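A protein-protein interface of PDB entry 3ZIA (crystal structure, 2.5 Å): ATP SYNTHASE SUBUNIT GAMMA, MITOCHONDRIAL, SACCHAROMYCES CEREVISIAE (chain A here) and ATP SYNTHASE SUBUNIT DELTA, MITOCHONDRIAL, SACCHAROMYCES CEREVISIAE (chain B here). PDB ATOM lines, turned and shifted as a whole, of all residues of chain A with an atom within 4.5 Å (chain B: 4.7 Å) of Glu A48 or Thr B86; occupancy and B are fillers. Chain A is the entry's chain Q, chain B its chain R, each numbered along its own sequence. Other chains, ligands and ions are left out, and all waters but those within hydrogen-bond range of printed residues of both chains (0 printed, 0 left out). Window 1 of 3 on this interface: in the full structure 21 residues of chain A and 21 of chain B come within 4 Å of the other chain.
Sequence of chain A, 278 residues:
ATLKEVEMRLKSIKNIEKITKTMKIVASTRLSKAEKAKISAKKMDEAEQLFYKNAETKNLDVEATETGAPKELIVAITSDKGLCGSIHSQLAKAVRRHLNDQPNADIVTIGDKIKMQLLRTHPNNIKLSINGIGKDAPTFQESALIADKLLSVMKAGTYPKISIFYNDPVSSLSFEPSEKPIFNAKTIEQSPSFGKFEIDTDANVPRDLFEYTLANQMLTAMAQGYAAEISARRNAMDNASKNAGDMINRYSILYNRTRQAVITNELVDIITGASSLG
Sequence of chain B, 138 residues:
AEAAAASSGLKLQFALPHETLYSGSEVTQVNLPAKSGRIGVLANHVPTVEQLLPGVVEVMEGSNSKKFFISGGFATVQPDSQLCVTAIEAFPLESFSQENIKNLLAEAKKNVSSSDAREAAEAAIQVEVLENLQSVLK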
ATOM      1  N   MET A  44      15.905  13.945  22.531  1.00  0.00           N
ATOM      2  CA  MET A  44      14.994  14.903  23.153  1.00  0.00           C
ATOM      3  C   MET A  44      13.552  14.397  23.010  1.00  0.00           C
ATOM      4  O   MET A  44      12.603  15.175  22.887  1.00  0.00           O
ATOM      5  CB  MET A  44      15.173  16.285  22.515  1.00  0.00           C
ATOM      6  CG  MET A  44      14.568  17.435  23.307  1.00  0.00           C
ATOM      7  SD  MET A  44      15.390  19.000  22.977  1.00  0.00           S
ATOM      8  CE  MET A  44      14.299  20.151  23.811  1.00  0.00           C
ATOM      9  N   ASP A  45      13.411  13.075  23.023  1.00  0.00           N
ATOM     10  CA  ASP A  45      12.123  12.400  22.943  1.00  0.00           C
ATOM     11  C   ASP A  45      12.122  11.258  23.958  1.00  0.00           C
ATOM     12  O   ASP A  45      11.073  10.876  24.484  1.00  0.00           O
ATOM     13  CB  ASP A  45      11.894  11.863  21.527  1.00  0.00           C
ATOM     14  CG  ASP A  45      10.431  11.568  21.235  1.00  0.00           C
ATOM     15  OD1 ASP A  45       9.548  12.251  21.797  1.00  0.00           O
ATOM     16  OD2 ASP A  45      10.163  10.655  20.424  1.00  0.00           O
ATOM     17  N   GLU A  46      13.314  10.720  24.217  1.00  0.00           N
ATOM     18  CA  GLU A  46      13.535   9.748  25.285  1.00  0.00           C
ATOM     19  C   GLU A  46      13.624  10.473  26.628  1.00  0.00           C
ATOM     20  O   GLU A  46      13.131   9.975  27.639  1.00  0.00           O
ATOM     21  CB  GLU A  46      14.819   8.941  25.037  1.00  0.00           C
ATOM     22  CG  GLU A  46      14.744   7.956  23.865  1.00  0.00           C
ATOM     23  CD  GLU A  46      16.083   7.289  23.548  1.00  0.00           C
ATOM     24  OE1 GLU A  46      17.148   7.845  23.907  1.00  0.00           O
ATOM     25  OE2 GLU A  46      16.068   6.206  22.926  1.00  0.00           O
ATOM     26  N   ALA A  47      14.248  11.651  26.619  1.00  0.00           N
ATOM     27  CA  ALA A  47      14.422  12.475  27.819  1.00  0.00           C
ATOM     28  C   ALA A  47      13.233  13.404  28.077  1.00  0.00           C
ATOM     29  O   ALA A  47      12.934  13.738  29.228  1.00  0.00           O
ATOM     30  CB  ALA A  47      15.716  13.282  27.723  1.00  0.00           C
ATOM     31  N   GLU A  48      12.564  13.815  27.005  1.00  0.00           N
ATOM     32  CA  GLU A  48      11.436  14.735  27.096  1.00  0.00           C
ATOM     33  C   GLU A  48      10.163  14.044  27.585  1.00  0.00           C
ATOM     34  O   GLU A  48       9.455  14.581  28.442  1.00  0.00           O
ATOM     35  CB  GLU A  48      11.205  15.431  25.745  1.00  0.00           C
ATOM     36  CG  GLU A  48       9.958  16.330  25.648  1.00  0.00           C
ATOM     37  CD  GLU A  48       9.979  17.533  26.588  1.00  0.00           C
ATOM     38  OE1 GLU A  48      11.017  17.794  27.243  1.00  0.00           O
ATOM     39  OE2 GLU A  48       8.940  18.220  26.666  1.00  0.00           O
ATOM     40  N   GLN A  49       9.884  12.858  27.042  1.00  0.00           N
ATOM     41  CA  GLN A  49       8.655  12.130  27.362  1.00  0.00           C
ATOM     42  C   GLN A  49       8.835  11.067  28.460  1.00  0.00           C
ATOM     43  O   GLN A  49       7.880  10.369  28.811  1.00  0.00           O
ATOM     44  CB  GLN A  49       8.036  11.515  26.095  1.00  0.00           C
ATOM     45  CG  GLN A  49       6.570  11.092  26.261  1.00  0.00           C
ATOM     46  CD  GLN A  49       5.993  10.355  25.064  1.00  0.00           C
ATOM     47  OE1 GLN A  49       6.525  10.419  23.956  1.00  0.00           O
ATOM     48  NE2 GLN A  49       4.884   9.654  25.287  1.00  0.00           N
ATOM     49  N   LEU A  50      10.045  10.953  29.009  1.00  0.00           N
ATOM     50  CA  LEU A  50      10.292  10.019  30.118  1.00  0.00           C
ATOM     51  C   LEU A  50       9.465  10.366  31.361  1.00  0.00           C
ATOM     52  O   LEU A  50       9.187   9.498  32.193  1.00  0.00           O
ATOM     53  CB  LEU A  50      11.783   9.939  30.462  1.00  0.00           C
ATOM     54  CG  LEU A  50      12.272   8.671  31.175  1.00  0.00           C
ATOM     55  CD1 LEU A  50      12.071   7.416  30.317  1.00  0.00           C
ATOM     56  CD2 LEU A  50      13.731   8.817  31.584  1.00  0.00           C
ATOM     57  N   PHE A  51       9.079  11.637  31.475  1.00  0.00           N
ATOM     58  CA  PHE A  51       8.096  12.076  32.460  1.00  0.00           C
ATOM     59  C   PHE A  51       6.742  11.403  32.218  1.00  0.00           C
ATOM     60  O   PHE A  51       6.073  10.999  33.166  1.00  0.00           O
ATOM     61  CB  PHE A  51       7.950  13.602  32.430  1.00  0.00           C
ATOM     62  CG  PHE A  51       6.659  14.104  33.026  1.00  0.00           C
ATOM     63  CD1 PHE A  51       6.546  14.323  34.397  1.00  0.00           C
ATOM     64  CD2 PHE A  51       5.553  14.355  32.214  1.00  0.00           C
ATOM     65  CE1 PHE A  51       5.351  14.783  34.951  1.00  0.00           C
ATOM     66  CE2 PHE A  51       4.354  14.812  32.758  1.00  0.00           C
ATOM     67  CZ  PHE A  51       4.253  15.029  34.127  1.00  0.00           C
ATOM     68  N   TYR A  52       6.348  11.293  30.950  1.00  0.00           N
ATOM     69  CA  TYR A  52       5.060  10.698  30.568  1.00  0.00           C
ATOM     70  C   TYR A  52       5.039   9.169  30.703  1.00  0.00           C
ATOM     71  O   TYR A  52       3.967   8.566  30.789  1.00  0.00           O
ATOM     72  CB  TYR A  52       4.676  11.100  29.135  1.00  0.00           C
ATOM     73  CG  TYR A  52       4.354  12.574  28.926  1.00  0.00           C
ATOM     74  CD1 TYR A  52       5.368  13.514  28.714  1.00  0.00           C
ATOM     75  CD2 TYR A  52       3.032  13.022  28.916  1.00  0.00           C
ATOM     76  CE1 TYR A  52       5.072  14.863  28.514  1.00  0.00           C
ATOM     77  CE2 TYR A  52       2.726  14.368  28.716  1.00  0.00           C
ATOM     78  CZ  TYR A  52       3.749  15.281  28.516  1.00  0.00           C
ATOM     79  OH  TYR A  52       3.444  16.609  28.316  1.00  0.00           O
ATOM     80  N   TYR A 212       5.128  23.085  25.984  1.00  0.00           N
ATOM     81  CA  TYR A 212       6.528  22.793  25.686  1.00  0.00           C
ATOM     82  C   TYR A 212       6.665  21.474  24.945  1.00  0.00           C
ATOM     83  O   TYR A 212       7.482  21.354  24.031  1.00  0.00           O
ATOM     84  CB  TYR A 212       7.328  22.744  26.985  1.00  0.00           C
ATOM     85  CG  TYR A 212       8.813  22.472  26.852  1.00  0.00           C
ATOM     86  CD1 TYR A 212       9.665  23.408  26.274  1.00  0.00           C
ATOM     87  CD2 TYR A 212       9.370  21.296  27.352  1.00  0.00           C
ATOM     88  CE1 TYR A 212      11.031  23.169  26.170  1.00  0.00           C
ATOM     89  CE2 TYR A 212      10.735  21.048  27.258  1.00  0.00           C
ATOM     90  CZ  TYR A 212      11.561  21.990  26.663  1.00  0.00           C
ATOM     91  OH  TYR A 212      12.916  21.760  26.563  1.00  0.00           O
ATOM     92  N   THR A 213       5.875  20.483  25.353  1.00  0.00           N
ATOM     93  CA  THR A 213       5.893  19.170  24.716  1.00  0.00           C
ATOM     94  C   THR A 213       5.262  19.257  23.328  1.00  0.00           C
ATOM     95  O   THR A 213       5.779  18.660  22.383  1.00  0.00           O
ATOM     96  CB  THR A 213       5.204  18.091  25.587  1.00  0.00           C
ATOM     97  OG1 THR A 213       5.769  18.115  26.905  1.00  0.00           O
ATOM     98  CG2 THR A 213       5.407  16.702  24.999  1.00  0.00           C
ATOM     99  N   ASN A 216       8.053  20.392  21.146  1.00  0.00           N
ATOM    100  CA  ASN A 216       9.127  19.416  20.987  1.00  0.00           C
ATOM    101  C   ASN A 216       8.714  18.201  20.174  1.00  0.00           C
ATOM    102  O   ASN A 216       9.493  17.707  19.356  1.00  0.00           O
ATOM    103  CB  ASN A 216       9.660  18.967  22.340  1.00  0.00           C
ATOM    104  CG  ASN A 216      10.618  19.962  22.942  1.00  0.00           C
ATOM    105  OD1 ASN A 216      11.523  20.460  22.270  1.00  0.00           O
ATOM    106  ND2 ASN A 216      10.427  20.259  24.219  1.00  0.00           N
ATOM    107  N   GLN A 217       7.496  17.721  20.408  1.00  0.00           N
ATOM    108  CA  GLN A 217       6.998  16.535  19.719  1.00  0.00           C
ATOM    109  C   GLN A 217       6.807  16.804  18.238  1.00  0.00           C
ATOM    110  O   GLN A 217       7.167  15.971  17.406  1.00  0.00           O
ATOM    111  CB  GLN A 217       5.699  16.018  20.352  1.00  0.00           C
ATOM    112  CG  GLN A 217       5.902  15.307  21.684  1.00  0.00           C
ATOM    113  CD  GLN A 217       6.931  14.191  21.613  1.00  0.00           C
ATOM    114  OE1 GLN A 217       6.697  13.149  20.996  1.00  0.00           O
ATOM    115  NE2 GLN A 217       8.081  14.405  22.252  1.00  0.00           N
ATOM    116  N   ALA B  15      20.312  17.370  26.646  1.00  0.00           N
ATOM    117  CA  ALA B  15      19.993  17.355  25.217  1.00  0.00           C
ATOM    118  C   ALA B  15      19.352  18.637  24.684  1.00  0.00           C
ATOM    119  O   ALA B  15      18.466  19.222  25.311  1.00  0.00           O
ATOM    120  CB  ALA B  15      19.112  16.152  24.888  1.00  0.00           C
ATOM    121  N   GLY B  72      16.703  28.181  28.329  1.00  0.00           N
ATOM    122  CA  GLY B  72      15.576  27.812  29.174  1.00  0.00           C
ATOM    123  C   GLY B  72      14.811  26.631  28.609  1.00  0.00           C
ATOM    124  O   GLY B  72      14.693  26.481  27.393  1.00  0.00           O
ATOM    125  N   GLY B  73      14.289  25.792  29.496  1.00  0.00           N
ATOM    126  CA  GLY B  73      13.515  24.627  29.092  1.00  0.00           C
ATOM    127  C   GLY B  73      12.789  24.002  30.262  1.00  0.00           C
ATOM    128  O   GLY B  73      11.965  24.654  30.905  1.00  0.00           O
ATOM    129  N   PHE B  74      13.101  22.734  30.526  1.00  0.00           N
ATOM    130  CA  PHE B  74      12.508  21.978  31.628  1.00  0.00           C
ATOM    131  C   PHE B  74      13.533  21.040  32.256  1.00  0.00           C
ATOM    132  O   PHE B  74      14.233  20.308  31.552  1.00  0.00           O
ATOM    133  CB  PHE B  74      11.289  21.177  31.149  1.00  0.00           C
ATOM    134  CG  PHE B  74       9.963  21.806  31.496  1.00  0.00           C
ATOM    135  CD1 PHE B  74       9.416  22.810  30.701  1.00  0.00           C
ATOM    136  CD2 PHE B  74       9.251  21.378  32.611  1.00  0.00           C
ATOM    137  CE1 PHE B  74       8.185  23.387  31.019  1.00  0.00           C
ATOM    138  CE2 PHE B  74       8.018  21.948  32.935  1.00  0.00           C
ATOM    139  CZ  PHE B  74       7.485  22.952  32.135  1.00  0.00           C
ATOM    140  N   CYS B  84      17.491  14.812  33.592  1.00  0.00           N
ATOM    141  CA  CYS B  84      17.238  15.128  32.193  1.00  0.00           C
ATOM    142  C   CYS B  84      16.971  16.618  32.035  1.00  0.00           C
ATOM    143  O   CYS B  84      15.953  17.139  32.497  1.00  0.00           O
ATOM    144  CB  CYS B  84      16.065  14.304  31.654  1.00  0.00           C
ATOM    145  SG  CYS B  84      16.305  12.515  31.777  1.00  0.00           S
ATOM    146  N   VAL B  85      17.910  17.300  31.393  1.00  0.00           N
ATOM    147  CA  VAL B  85      17.799  18.734  31.175  1.00  0.00           C
ATOM    148  C   VAL B  85      17.680  19.004  29.680  1.00  0.00           C
ATOM    149  O   VAL B  85      18.580  18.670  28.903  1.00  0.00           O
ATOM    150  CB  VAL B  85      19.004  19.492  31.779  1.00  0.00           C
ATOM    151  CG1 VAL B  85      18.883  20.986  31.526  1.00  0.00           C
ATOM    152  CG2 VAL B  85      19.114  19.216  33.273  1.00  0.00           C
ATOM    153  N   THR B  86      16.554  19.593  29.287  1.00  0.00           N
ATOM    154  CA  THR B  86      16.282  19.900  27.885  1.00  0.00           C
ATOM    155  C   THR B  86      16.222  21.408  27.662  1.00  0.00           C
ATOM    156  O   THR B  86      15.439  22.107  28.308  1.00  0.00           O
ATOM    157  CB  THR B  86      14.962  19.255  27.391  1.00  0.00           C
ATOM    158  OG1 THR B  86      13.841  19.900  28.008  1.00  0.00           O
ATOM    159  CG2 THR B  86      14.925  17.766  27.700  1.00  0.00           C
ATOM    160  N   ALA B  87      17.055  21.898  26.747  1.00  0.00           N
ATOM    161  CA  ALA B  87      17.065  23.314  26.379  1.00  0.00           C
ATOM    162  C   ALA B  87      17.221  23.479  24.874  1.00  0.00           C
ATOM    163  O   ALA B  87      17.864  22.660  24.222  1.00  0.00           O
ATOM    164  CB  ALA B  87      18.178  24.050  27.111  1.00  0.00           C
ATOM    165  N   ILE B  88      16.632  24.546  24.341  1.00  0.00           N
ATOM    166  CA  ILE B  88      16.702  24.865  22.915  1.00  0.00           C
ATOM    167  C   ILE B  88      18.114  25.280  22.494  1.00  0.00           C
ATOM    168  O   ILE B  88      18.679  24.704  21.566  1.00  0.00           O
ATOM    169  CB  ILE B  88      15.671  25.941  22.543  1.00  0.00           C
ATOM    170  CG1 ILE B  88      14.268  25.413  22.819  1.00  0.00           C
ATOM    171  CG2 ILE B  88      15.795  26.341  21.084  1.00  0.00           C
ATOM    172  CD1 ILE B  88      13.437  26.354  23.622  1.00  0.00           C
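The side-chain hydroxyl of Tyr A212 is in hydrogen-bond range of the side-chain hydroxyl of Thr B86 (2.5 Å).
O of Tyr A212 lies within hydrogen-bond range of ND2 of Asn A216. The backbone carbonyl oxygen (O) of Thr B86 sits at hydrogen-bond distance from the backbone NH (N) of Phe B74. The backbone NH of Ala B15 sits at hydrogen-bond distance from the backbone carbonyl oxygen of Val B85 (3.1 Å). OG1 of Thr A213 is in hydrogen-bond range of OE2 of Glu A48 (3.2 Å). The backbone carbonyl oxygen (O) of Ala B15 sits at hydrogen-bond distance from the backbone NH (N) of Ala B87 (3.3 Å).
Ala B15 touches Met A44. Met A44 touches Thr B86 (CE to CB, 3.7 Å). Glu A48 touches Thr B86 (OE1 to OG1, 3.6 Å). OH of Tyr A212 touches CA of Gly B73, at 3.9 Å. CD2 of Tyr A212 touches CD1 of Phe B74 (3.7 Å).
Glu A48 touches one residue of chain B. Thr B86 touches three residues of chain A. Printed residues of chain A within 4 Å of Phe B74: Tyr A212. Printed residues of chain A within 4 Å of Ala B15: Met A44 (3.9 Å). Printed residues of chain B within 4 Å of Tyr A212: Gly B73 (3.9 Å), Phe B74 (3.7 Å) and Thr B86 (2.5 Å). Of the printed residues of chain A, Gly B73 touches Tyr A212 (3.9 Å). Printed residues of chain B within 4 Å of Met A44: Ala B15 (3.9 Å) and Thr B86 (3.7 Å). Gln A49 touches none of the printed residues of chain B. The nearest printed residue of chain B that does not touch Glu A48 is Phe B74 (5.2 Å). The nearest printed residue of chain A that does not touch Thr B86 is Ala A47 (4.6 Å).
Among the printed residues, no Asp or Glu carboxylate lies within 4 Å of a Lys or Arg side-chain nitrogen of the other chain.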
